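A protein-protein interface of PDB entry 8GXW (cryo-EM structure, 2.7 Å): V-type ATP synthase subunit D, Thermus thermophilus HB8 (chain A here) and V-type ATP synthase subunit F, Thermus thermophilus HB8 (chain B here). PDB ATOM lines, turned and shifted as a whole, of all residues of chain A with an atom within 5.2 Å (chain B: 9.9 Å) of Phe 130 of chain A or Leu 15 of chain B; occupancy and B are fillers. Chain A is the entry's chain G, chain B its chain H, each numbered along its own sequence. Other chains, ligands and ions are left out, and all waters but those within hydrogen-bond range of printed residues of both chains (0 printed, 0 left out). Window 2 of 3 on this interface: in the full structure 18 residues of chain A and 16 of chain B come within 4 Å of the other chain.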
ATOM      1  N   ALA A  60     -15.478 -18.219 -12.212  1.00  0.00           N
ATOM      2  CA  ALA A  60     -16.375 -18.173 -13.361  1.00  0.00           C
ATOM      3  C   ALA A  60     -17.798 -17.831 -12.936  1.00  0.00           C
ATOM      4  O   ALA A  60     -18.474 -17.024 -13.587  1.00  0.00           O
ATOM      5  CB  ALA A  60     -16.344 -19.508 -14.105  1.00  0.00           C
ATOM      6  N   TYR A  61     -18.274 -18.439 -11.847  1.00  0.00           N
ATOM      7  CA  TYR A  61     -19.613 -18.130 -11.360  1.00  0.00           C
ATOM      8  C   TYR A  61     -19.706 -16.679 -10.908  1.00  0.00           C
ATOM      9  O   TYR A  61     -20.707 -16.002 -11.170  1.00  0.00           O
ATOM     10  CB  TYR A  61     -19.986 -19.075 -10.217  1.00  0.00           C
ATOM     11  CG  TYR A  61     -20.163 -20.522 -10.629  1.00  0.00           C
ATOM     12  CD1 TYR A  61     -20.330 -20.877 -11.963  1.00  0.00           C
ATOM     13  CD2 TYR A  61     -20.169 -21.535  -9.680  1.00  0.00           C
ATOM     14  CE1 TYR A  61     -20.493 -22.198 -12.337  1.00  0.00           C
ATOM     15  CE2 TYR A  61     -20.331 -22.858 -10.044  1.00  0.00           C
ATOM     16  CZ  TYR A  61     -20.494 -23.183 -11.374  1.00  0.00           C
ATOM     17  OH  TYR A  61     -20.655 -24.499 -11.742  1.00  0.00           O
ATOM     18  N   LEU A  64     -20.013 -14.573 -14.021  1.00  0.00           N
ATOM     19  CA  LEU A  64     -21.302 -14.678 -14.700  1.00  0.00           C
ATOM     20  C   LEU A  64     -22.426 -14.045 -13.888  1.00  0.00           C
ATOM     21  O   LEU A  64     -23.427 -13.602 -14.464  1.00  0.00           O
ATOM     22  CB  LEU A  64     -21.637 -16.141 -14.990  1.00  0.00           C
ATOM     23  CG  LEU A  64     -22.879 -16.346 -15.871  1.00  0.00           C
ATOM     24  CD1 LEU A  64     -22.491 -16.326 -17.344  1.00  0.00           C
ATOM     25  CD2 LEU A  64     -23.632 -17.628 -15.525  1.00  0.00           C
ATOM     26  N   VAL A  76     -29.303 -11.991 -22.749  1.00  0.00           N
ATOM     27  CA  VAL A  76     -28.194 -12.904 -22.483  1.00  0.00           C
ATOM     28  C   VAL A  76     -28.532 -14.305 -22.977  1.00  0.00           C
ATOM     29  O   VAL A  76     -27.691 -14.990 -23.570  1.00  0.00           O
ATOM     30  CB  VAL A  76     -27.848 -12.901 -20.982  1.00  0.00           C
ATOM     31  CG1 VAL A  76     -26.815 -13.974 -20.670  1.00  0.00           C
ATOM     32  CG2 VAL A  76     -27.348 -11.530 -20.555  1.00  0.00           C
ATOM     33  N   ALA A  80     -26.565 -16.399 -25.835  1.00  0.00           N
ATOM     34  CA  ALA A  80     -26.097 -17.760 -25.597  1.00  0.00           C
ATOM     35  C   ALA A  80     -26.613 -18.712 -26.666  1.00  0.00           C
ATOM     36  O   ALA A  80     -25.860 -19.545 -27.184  1.00  0.00           O
ATOM     37  CB  ALA A  80     -26.539 -18.226 -24.212  1.00  0.00           C
ATOM     38  N   THR A 123     -21.482 -10.130 -21.481  1.00  0.00           N
ATOM     39  CA  THR A 123     -21.711 -11.550 -21.731  1.00  0.00           C
ATOM     40  C   THR A 123     -20.535 -12.182 -22.465  1.00  0.00           C
ATOM     41  O   THR A 123     -20.124 -13.302 -22.144  1.00  0.00           O
ATOM     42  CB  THR A 123     -22.998 -11.743 -22.532  1.00  0.00           C
ATOM     43  OG1 THR A 123     -24.116 -11.272 -21.768  1.00  0.00           O
ATOM     44  CG2 THR A 123     -23.205 -13.213 -22.869  1.00  0.00           C
ATOM     45  N   ALA A 126     -17.653 -13.222 -20.281  1.00  0.00           N
ATOM     46  CA  ALA A 126     -17.935 -14.379 -19.438  1.00  0.00           C
ATOM     47  C   ALA A 126     -17.692 -15.697 -20.161  1.00  0.00           C
ATOM     48  O   ALA A 126     -17.546 -16.733 -19.503  1.00  0.00           O
ATOM     49  CB  ALA A 126     -19.380 -14.320 -18.941  1.00  0.00           C
ATOM     50  N   SER A 127     -17.649 -15.686 -21.495  1.00  0.00           N
ATOM     51  CA  SER A 127     -17.417 -16.924 -22.233  1.00  0.00           C
ATOM     52  C   SER A 127     -16.048 -17.511 -21.909  1.00  0.00           C
ATOM     53  O   SER A 127     -15.912 -18.727 -21.736  1.00  0.00           O
ATOM     54  CB  SER A 127     -17.550 -16.670 -23.734  1.00  0.00           C
ATOM     55  OG  SER A 127     -17.456 -17.879 -24.466  1.00  0.00           O
ATOM     56  N   ARG A 128     -15.023 -16.660 -21.819  1.00  0.00           N
ATOM     57  CA  ARG A 128     -13.676 -17.148 -21.538  1.00  0.00           C
ATOM     58  C   ARG A 128     -13.616 -17.848 -20.185  1.00  0.00           C
ATOM     59  O   ARG A 128     -12.938 -18.873 -20.032  1.00  0.00           O
ATOM     60  CB  ARG A 128     -12.685 -15.985 -21.585  1.00  0.00           C
ATOM     61  CG  ARG A 128     -11.219 -16.403 -21.548  1.00  0.00           C
ATOM     62  CD  ARG A 128     -10.645 -16.582 -22.947  1.00  0.00           C
ATOM     63  NE  ARG A 128     -10.793 -17.950 -23.431  1.00  0.00           N
ATOM     64  CZ  ARG A 128     -10.708 -18.310 -24.704  1.00  0.00           C
ATOM     65  NH1 ARG A 128     -10.472 -17.425 -25.660  1.00  0.00           N
ATOM     66  NH2 ARG A 128     -10.862 -19.590 -25.028  1.00  0.00           N
ATOM     67  N   ALA A 129     -14.310 -17.298 -19.186  1.00  0.00           N
ATOM     68  CA  ALA A 129     -14.310 -17.915 -17.865  1.00  0.00           C
ATOM     69  C   ALA A 129     -14.884 -19.323 -17.918  1.00  0.00           C
ATOM     70  O   ALA A 129     -14.331 -20.251 -17.316  1.00  0.00           O
ATOM     71  CB  ALA A 129     -15.101 -17.050 -16.884  1.00  0.00           C
ATOM     72  N   PHE A 130     -15.985 -19.511 -18.648  1.00  0.00           N
ATOM     73  CA  PHE A 130     -16.568 -20.844 -18.743  1.00  0.00           C
ATOM     74  C   PHE A 130     -15.724 -21.767 -19.609  1.00  0.00           C
ATOM     75  O   PHE A 130     -15.723 -22.979 -19.386  1.00  0.00           O
ATOM     76  CB  PHE A 130     -17.997 -20.764 -19.285  1.00  0.00           C
ATOM     77  CG  PHE A 130     -19.038 -20.414 -18.244  1.00  0.00           C
ATOM     78  CD1 PHE A 130     -18.742 -20.424 -16.885  1.00  0.00           C
ATOM     79  CD2 PHE A 130     -20.325 -20.087 -18.634  1.00  0.00           C
ATOM     80  CE1 PHE A 130     -19.702 -20.108 -15.949  1.00  0.00           C
ATOM     81  CE2 PHE A 130     -21.289 -19.770 -17.697  1.00  0.00           C
ATOM     82  CZ  PHE A 130     -20.975 -19.782 -16.352  1.00  0.00           C
ATOM     83  N   ARG A 131     -14.998 -21.230 -20.591  1.00  0.00           N
ATOM     84  CA  ARG A 131     -14.058 -22.068 -21.329  1.00  0.00           C
ATOM     85  C   ARG A 131     -12.966 -22.599 -20.407  1.00  0.00           C
ATOM     86  O   ARG A 131     -12.628 -23.790 -20.445  1.00  0.00           O
ATOM     87  CB  ARG A 131     -13.448 -21.282 -22.490  1.00  0.00           C
ATOM     88  CG  ARG A 131     -14.460 -20.795 -23.523  1.00  0.00           C
ATOM     89  CD  ARG A 131     -14.886 -21.900 -24.476  1.00  0.00           C
ATOM     90  NE  ARG A 131     -15.830 -22.821 -23.856  1.00  0.00           N
ATOM     91  CZ  ARG A 131     -17.103 -22.540 -23.612  1.00  0.00           C
ATOM     92  NH1 ARG A 131     -17.627 -21.368 -23.930  1.00  0.00           N
ATOM     93  NH2 ARG A 131     -17.870 -23.458 -23.030  1.00  0.00           N
ATOM     94  N   ARG A 132     -12.415 -21.730 -19.557  1.00  0.00           N
ATOM     95  CA  ARG A 132     -11.418 -22.179 -18.589  1.00  0.00           C
ATOM     96  C   ARG A 132     -12.022 -23.172 -17.599  1.00  0.00           C
ATOM     97  O   ARG A 132     -11.373 -24.151 -17.211  1.00  0.00           O
ATOM     98  CB  ARG A 132     -10.821 -20.978 -17.856  1.00  0.00           C
ATOM     99  CG  ARG A 132     -10.116 -19.990 -18.772  1.00  0.00           C
ATOM    100  CD  ARG A 132      -9.481 -18.849 -17.992  1.00  0.00           C
ATOM    101  NE  ARG A 132     -10.475 -17.989 -17.358  1.00  0.00           N
ATOM    102  CZ  ARG A 132     -10.911 -18.128 -16.113  1.00  0.00           C
ATOM    103  NH1 ARG A 132     -10.478 -19.103 -15.330  1.00  0.00           N
ATOM    104  NH2 ARG A 132     -11.808 -17.266 -15.641  1.00  0.00           N
ATOM    105  N   TYR A 133     -13.264 -22.933 -17.178  1.00  0.00           N
ATOM    106  CA  TYR A 133     -13.931 -23.864 -16.274  1.00  0.00           C
ATOM    107  C   TYR A 133     -14.114 -25.229 -16.925  1.00  0.00           C
ATOM    108  O   TYR A 133     -13.942 -26.264 -16.276  1.00  0.00           O
ATOM    109  CB  TYR A 133     -15.281 -23.292 -15.846  1.00  0.00           C
ATOM    110  CG  TYR A 133     -16.210 -24.310 -15.233  1.00  0.00           C
ATOM    111  CD1 TYR A 133     -16.017 -24.762 -13.937  1.00  0.00           C
ATOM    112  CD2 TYR A 133     -17.280 -24.820 -15.953  1.00  0.00           C
ATOM    113  CE1 TYR A 133     -16.864 -25.692 -13.373  1.00  0.00           C
ATOM    114  CE2 TYR A 133     -18.134 -25.753 -15.398  1.00  0.00           C
ATOM    115  CZ  TYR A 133     -17.922 -26.185 -14.108  1.00  0.00           C
ATOM    116  OH  TYR A 133     -18.769 -27.115 -13.549  1.00  0.00           O
ATOM    117  N   ALA A 134     -14.481 -25.249 -18.208  1.00  0.00           N
ATOM    118  CA  ALA A 134     -14.620 -26.514 -18.920  1.00  0.00           C
ATOM    119  C   ALA A 134     -13.279 -27.219 -19.044  1.00  0.00           C
ATOM    120  O   ALA A 134     -13.202 -28.447 -18.932  1.00  0.00           O
ATOM    121  CB  ALA A 134     -15.229 -26.274 -20.300  1.00  0.00           C
ATOM    122  N   GLU A 135     -12.209 -26.461 -19.288  1.00  0.00           N
ATOM    123  CA  GLU A 135     -10.882 -27.067 -19.317  1.00  0.00           C
ATOM    124  C   GLU A 135     -10.549 -27.701 -17.971  1.00  0.00           C
ATOM    125  O   GLU A 135     -10.011 -28.813 -17.911  1.00  0.00           O
ATOM    126  CB  GLU A 135      -9.834 -26.022 -19.695  1.00  0.00           C
ATOM    127  CG  GLU A 135      -9.946 -25.521 -21.127  1.00  0.00           C
ATOM    128  CD  GLU A 135      -9.517 -26.561 -22.145  1.00  0.00           C
ATOM    129  OE1 GLU A 135      -8.626 -27.376 -21.827  1.00  0.00           O
ATOM    130  OE2 GLU A 135     -10.072 -26.561 -23.264  1.00  0.00           O
ATOM    131  N   MET B   1     -20.967 -31.993 -23.788  1.00  0.00           N
ATOM    132  CA  MET B   1     -21.079 -32.544 -22.408  1.00  0.00           C
ATOM    133  C   MET B   1     -22.415 -32.134 -21.796  1.00  0.00           C
ATOM    134  O   MET B   1     -22.960 -31.083 -22.133  1.00  0.00           O
ATOM    135  CB  MET B   1     -19.916 -32.051 -21.547  1.00  0.00           C
ATOM    136  CG  MET B   1     -18.553 -32.511 -22.042  1.00  0.00           C
ATOM    137  SD  MET B   1     -17.182 -31.629 -21.275  1.00  0.00           S
ATOM    138  CE  MET B   1     -17.269 -32.265 -19.607  1.00  0.00           C
ATOM    139  N   PRO B   7     -32.645 -25.697 -12.200  1.00  0.00           N
ATOM    140  CA  PRO B   7     -32.918 -24.949 -13.439  1.00  0.00           C
ATOM    141  C   PRO B   7     -32.088 -23.686 -13.583  1.00  0.00           C
ATOM    142  O   PRO B   7     -31.742 -23.310 -14.710  1.00  0.00           O
ATOM    143  CB  PRO B   7     -34.417 -24.627 -13.334  1.00  0.00           C
ATOM    144  CG  PRO B   7     -34.961 -25.592 -12.334  1.00  0.00           C
ATOM    145  CD  PRO B   7     -33.851 -25.852 -11.370  1.00  0.00           C
ATOM    146  N   GLU B   8     -31.755 -23.017 -12.476  1.00  0.00           N
ATOM    147  CA  GLU B   8     -31.043 -21.747 -12.568  1.00  0.00           C
ATOM    148  C   GLU B   8     -29.656 -21.913 -13.180  1.00  0.00           C
ATOM    149  O   GLU B   8     -29.216 -21.049 -13.945  1.00  0.00           O
ATOM    150  CB  GLU B   8     -30.937 -21.106 -11.185  1.00  0.00           C
ATOM    151  CG  GLU B   8     -32.270 -20.637 -10.625  1.00  0.00           C
ATOM    152  CD  GLU B   8     -32.143 -20.038  -9.239  1.00  0.00           C
ATOM    153  OE1 GLU B   8     -31.056 -20.154  -8.636  1.00  0.00           O
ATOM    154  OE2 GLU B   8     -33.131 -19.450  -8.752  1.00  0.00           O
ATOM    155  N   THR B   9     -28.951 -22.995 -12.851  1.00  0.00           N
ATOM    156  CA  THR B   9     -27.636 -23.240 -13.430  1.00  0.00           C
ATOM    157  C   THR B   9     -27.700 -23.990 -14.754  1.00  0.00           C
ATOM    158  O   THR B   9     -26.700 -24.020 -15.480  1.00  0.00           O
ATOM    159  CB  THR B   9     -26.759 -24.025 -12.447  1.00  0.00           C
ATOM    160  OG1 THR B   9     -25.394 -23.983 -12.881  1.00  0.00           O
ATOM    161  CG2 THR B   9     -27.214 -25.475 -12.352  1.00  0.00           C
ATOM    162  N   ALA B  10     -28.845 -24.593 -15.083  1.00  0.00           N
ATOM    163  CA  ALA B  10     -28.974 -25.275 -16.367  1.00  0.00           C
ATOM    164  C   ALA B  10     -28.844 -24.293 -17.524  1.00  0.00           C
ATOM    165  O   ALA B  10     -28.181 -24.585 -18.527  1.00  0.00           O
ATOM    166  CB  ALA B  10     -30.310 -26.013 -16.435  1.00  0.00           C
ATOM    167  N   GLN B  11     -29.475 -23.123 -17.406  1.00  0.00           N
ATOM    168  CA  GLN B  11     -29.337 -22.106 -18.442  1.00  0.00           C
ATOM    169  C   GLN B  11     -27.893 -21.629 -18.549  1.00  0.00           C
ATOM    170  O   GLN B  11     -27.399 -21.367 -19.649  1.00  0.00           O
ATOM    171  CB  GLN B  11     -30.275 -20.931 -18.161  1.00  0.00           C
ATOM    172  CG  GLN B  11     -30.079 -20.282 -16.801  1.00  0.00           C
ATOM    173  CD  GLN B  11     -31.194 -19.318 -16.448  1.00  0.00           C
ATOM    174  OE1 GLN B  11     -32.157 -19.162 -17.199  1.00  0.00           O
ATOM    175  NE2 GLN B  11     -31.072 -18.668 -15.297  1.00  0.00           N
ATOM    176  N   GLY B  12     -27.200 -21.511 -17.415  1.00  0.00           N
ATOM    177  CA  GLY B  12     -25.792 -21.147 -17.462  1.00  0.00           C
ATOM    178  C   GLY B  12     -24.949 -22.183 -18.181  1.00  0.00           C
ATOM    179  O   GLY B  12     -24.080 -21.842 -18.988  1.00  0.00           O
ATOM    180  N   PHE B  13     -25.194 -23.465 -17.900  1.00  0.00           N
ATOM    181  CA  PHE B  13     -24.464 -24.520 -18.595  1.00  0.00           C
ATOM    182  C   PHE B  13     -24.766 -24.500 -20.088  1.00  0.00           C
ATOM    183  O   PHE B  13     -23.868 -24.700 -20.914  1.00  0.00           O
ATOM    184  CB  PHE B  13     -24.809 -25.882 -17.993  1.00  0.00           C
ATOM    185  CG  PHE B  13     -24.037 -26.204 -16.743  1.00  0.00           C
ATOM    186  CD1 PHE B  13     -22.658 -26.335 -16.780  1.00  0.00           C
ATOM    187  CD2 PHE B  13     -24.689 -26.373 -15.534  1.00  0.00           C
ATOM    188  CE1 PHE B  13     -21.945 -26.629 -15.634  1.00  0.00           C
ATOM    189  CE2 PHE B  13     -23.981 -26.668 -14.384  1.00  0.00           C
ATOM    190  CZ  PHE B  13     -22.607 -26.796 -14.434  1.00  0.00           C
ATOM    191  N   ARG B  14     -26.027 -24.261 -20.455  1.00  0.00           N
ATOM    192  CA  ARG B  14     -26.367 -24.127 -21.868  1.00  0.00           C
ATOM    193  C   ARG B  14     -25.626 -22.953 -22.493  1.00  0.00           C
ATOM    194  O   ARG B  14     -25.165 -23.036 -23.638  1.00  0.00           O
ATOM    195  CB  ARG B  14     -27.880 -23.961 -22.029  1.00  0.00           C
ATOM    196  CG  ARG B  14     -28.357 -23.856 -23.475  1.00  0.00           C
ATOM    197  CD  ARG B  14     -28.100 -25.137 -24.256  1.00  0.00           C
ATOM    198  NE  ARG B  14     -28.849 -26.269 -23.721  1.00  0.00           N
ATOM    199  CZ  ARG B  14     -30.142 -26.479 -23.928  1.00  0.00           C
ATOM    200  NH1 ARG B  14     -30.872 -25.648 -24.654  1.00  0.00           N
ATOM    201  NH2 ARG B  14     -30.718 -27.551 -23.391  1.00  0.00           N
ATOM    202  N   LEU B  15     -25.504 -21.847 -21.755  1.00  0.00           N
ATOM    203  CA  LEU B  15     -24.711 -20.719 -22.229  1.00  0.00           C
ATOM    204  C   LEU B  15     -23.263 -21.132 -22.449  1.00  0.00           C
ATOM    205  O   LEU B  15     -22.621 -20.690 -23.408  1.00  0.00           O
ATOM    206  CB  LEU B  15     -24.797 -19.565 -21.227  1.00  0.00           C
ATOM    207  CG  LEU B  15     -24.042 -18.279 -21.573  1.00  0.00           C
ATOM    208  CD1 LEU B  15     -24.820 -17.061 -21.095  1.00  0.00           C
ATOM    209  CD2 LEU B  15     -22.642 -18.283 -20.972  1.00  0.00           C
ATOM    210  N   ALA B  16     -22.734 -21.983 -21.569  1.00  0.00           N
ATOM    211  CA  ALA B  16     -21.389 -22.513 -21.748  1.00  0.00           C
ATOM    212  C   ALA B  16     -21.281 -23.444 -22.948  1.00  0.00           C
ATOM    213  O   ALA B  16     -20.163 -23.798 -23.335  1.00  0.00           O
ATOM    214  CB  ALA B  16     -20.945 -23.251 -20.484  1.00  0.00           C
ATOM    215  N   GLY B  17     -22.405 -23.849 -23.540  1.00  0.00           N
ATOM    216  CA  GLY B  17     -22.412 -24.746 -24.675  1.00  0.00           C
ATOM    217  C   GLY B  17     -22.746 -26.183 -24.340  1.00  0.00           C
ATOM    218  O   GLY B  17     -22.876 -27.001 -25.260  1.00  0.00           O
ATOM    219  N   LEU B  18     -22.889 -26.515 -23.061  1.00  0.00           N
ATOM    220  CA  LEU B  18     -23.240 -27.861 -22.640  1.00  0.00           C
ATOM    221  C   LEU B  18     -24.761 -28.016 -22.669  1.00  0.00           C
ATOM    222  O   LEU B  18     -25.490 -27.123 -23.106  1.00  0.00           O
ATOM    223  CB  LEU B  18     -22.659 -28.143 -21.256  1.00  0.00           C
ATOM    224  CG  LEU B  18     -21.173 -28.505 -21.222  1.00  0.00           C
ATOM    225  CD1 LEU B  18     -20.309 -27.284 -21.497  1.00  0.00           C
ATOM    226  CD2 LEU B  18     -20.808 -29.130 -19.884  1.00  0.00           C
ATOM    227  N   GLU B  19     -25.254 -29.161 -22.207  1.00  0.00           N
ATOM    228  CA  GLU B  19     -26.683 -29.426 -22.111  1.00  0.00           C
ATOM    229  C   GLU B  19     -27.090 -29.422 -20.644  1.00  0.00           C
ATOM    230  O   GLU B  19     -26.532 -30.175 -19.838  1.00  0.00           O
ATOM    231  CB  GLU B  19     -27.038 -30.765 -22.758  1.00  0.00           C
ATOM    232  CG  GLU B  19     -27.034 -30.736 -24.278  1.00  0.00           C
ATOM    233  CD  GLU B  19     -27.588 -32.009 -24.887  1.00  0.00           C
ATOM    234  OE1 GLU B  19     -27.857 -32.964 -24.129  1.00  0.00           O
ATOM    235  OE2 GLU B  19     -27.754 -32.055 -26.124  1.00  0.00           O
ATOM    236  N   GLY B  20     -28.054 -28.583 -20.306  1.00  0.00           N
ATOM    237  CA  GLY B  20     -28.505 -28.450 -18.929  1.00  0.00           C
ATOM    238  C   GLY B  20     -29.992 -28.684 -18.807  1.00  0.00           C
ATOM    239  O   GLY B  20     -30.767 -28.303 -19.684  1.00  0.00           O
ATOM    240  N   TYR B  21     -30.384 -29.320 -17.705  1.00  0.00           N
ATOM    241  CA  TYR B  21     -31.782 -29.614 -17.429  1.00  0.00           C
ATOM    242  C   TYR B  21     -32.060 -29.383 -15.951  1.00  0.00           C
ATOM    243  O   TYR B  21     -31.235 -29.716 -15.096  1.00  0.00           O
ATOM    244  CB  TYR B  21     -32.133 -31.055 -17.809  1.00  0.00           C
ATOM    245  CG  TYR B  21     -31.760 -31.424 -19.228  1.00  0.00           C
ATOM    246  CD1 TYR B  21     -32.447 -30.890 -20.309  1.00  0.00           C
ATOM    247  CD2 TYR B  21     -30.718 -32.306 -19.485  1.00  0.00           C
ATOM    248  CE1 TYR B  21     -32.109 -31.223 -21.607  1.00  0.00           C
ATOM    249  CE2 TYR B  21     -30.371 -32.646 -20.779  1.00  0.00           C
ATOM    250  CZ  TYR B  21     -31.070 -32.102 -21.835  1.00  0.00           C
ATOM    251  OH  TYR B  21     -30.729 -32.438 -23.125  1.00  0.00           O
ATOM    252  N   LEU B  77     -24.788 -26.204  -5.950  1.00  0.00           N
ATOM    253  CA  LEU B  77     -24.825 -24.752  -6.080  1.00  0.00           C
ATOM    254  C   LEU B  77     -24.843 -24.079  -4.714  1.00  0.00           C
ATOM    255  O   LEU B  77     -24.053 -23.163  -4.450  1.00  0.00           O
ATOM    256  CB  LEU B  77     -26.045 -24.331  -6.903  1.00  0.00           C
ATOM    257  CG  LEU B  77     -26.250 -25.065  -8.230  1.00  0.00           C
ATOM    258  CD1 LEU B  77     -27.594 -24.695  -8.838  1.00  0.00           C
ATOM    259  CD2 LEU B  77     -25.117 -24.758  -9.196  1.00  0.00           C
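Printed residues of chain A that touch a printed residue of chain B: Val 76, Ala 80, Phe 130, Arg 131 and Tyr 133. Hydrophobic or aromatic side chains of chain A that line the printed part of chain B: Val 76, Ala 80, Phe 130 and Tyr 133. Of the 17 printed residues of chain B, 4 touch a printed residue of chain A. Hydrophobic or aromatic side chains of chain B within 4 Å of the printed part of chain A: Phe 13, Leu 15 and Ala 16. Among the printed residues, no Asp or Glu carboxylate lies within 4 Å of a Lys or Arg side-chain nitrogen of the other chain.
The backbone NH (N) of Leu 18 of chain B lies within hydrogen-bond range of the backbone carbonyl oxygen (O) of Phe 13 of chain B.
Among the printed residues, pairs that only touch across the chains: Ala 80 of chain A with Leu 15 of chain B (3.6 Å), Val 76 of chain A with Leu 15 of chain B (3.7 Å), Phe 130 of chain A with Gly 12 of chain B (3.7 Å), Phe 130 of chain A with Ala 16 of chain B (3.7 Å), Phe 130 of chain A with Leu 15 of chain B (3.8 Å) and Tyr 133 of chain A with Phe 13 of chain B (3.8 Å).
Leu 15 of chain B touches three residues of chain A. Of chain B, only Leu 15 comes within 4 Å of Ala 80 of chain A. No residue of chain B comes within 4 Å of Ala 129 of chain A. Arg 131 of chain A touches just one residue of chain B: Ala 16. Printed residues of chain A within 4 Å of Phe 13 of chain B: Tyr 133. Of the printed residues of chain A, Gly 12 of chain B touches Phe 130. Of the printed residues of chain A, Ala 16 of chain B touches Phe 130 (3.7 Å) and Arg 131 (2.3 Å). Printed residues of chain B within 4 Å of Val 76 of chain A: Leu 15 (3.7 Å). Of the printed residues of chain B, Tyr 133 of chain A touches Phe 13 (3.8 Å). Glu 135 of chain A touches none of the printed residues of chain B. The nearest printed residue of chain B that does not touch Val 76 of chain A is Gln 11 of chain B (7.5 Å).
O of Ala 16 of chain B lies close to NH2 of Arg 131 of chain A (2.3 Å).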
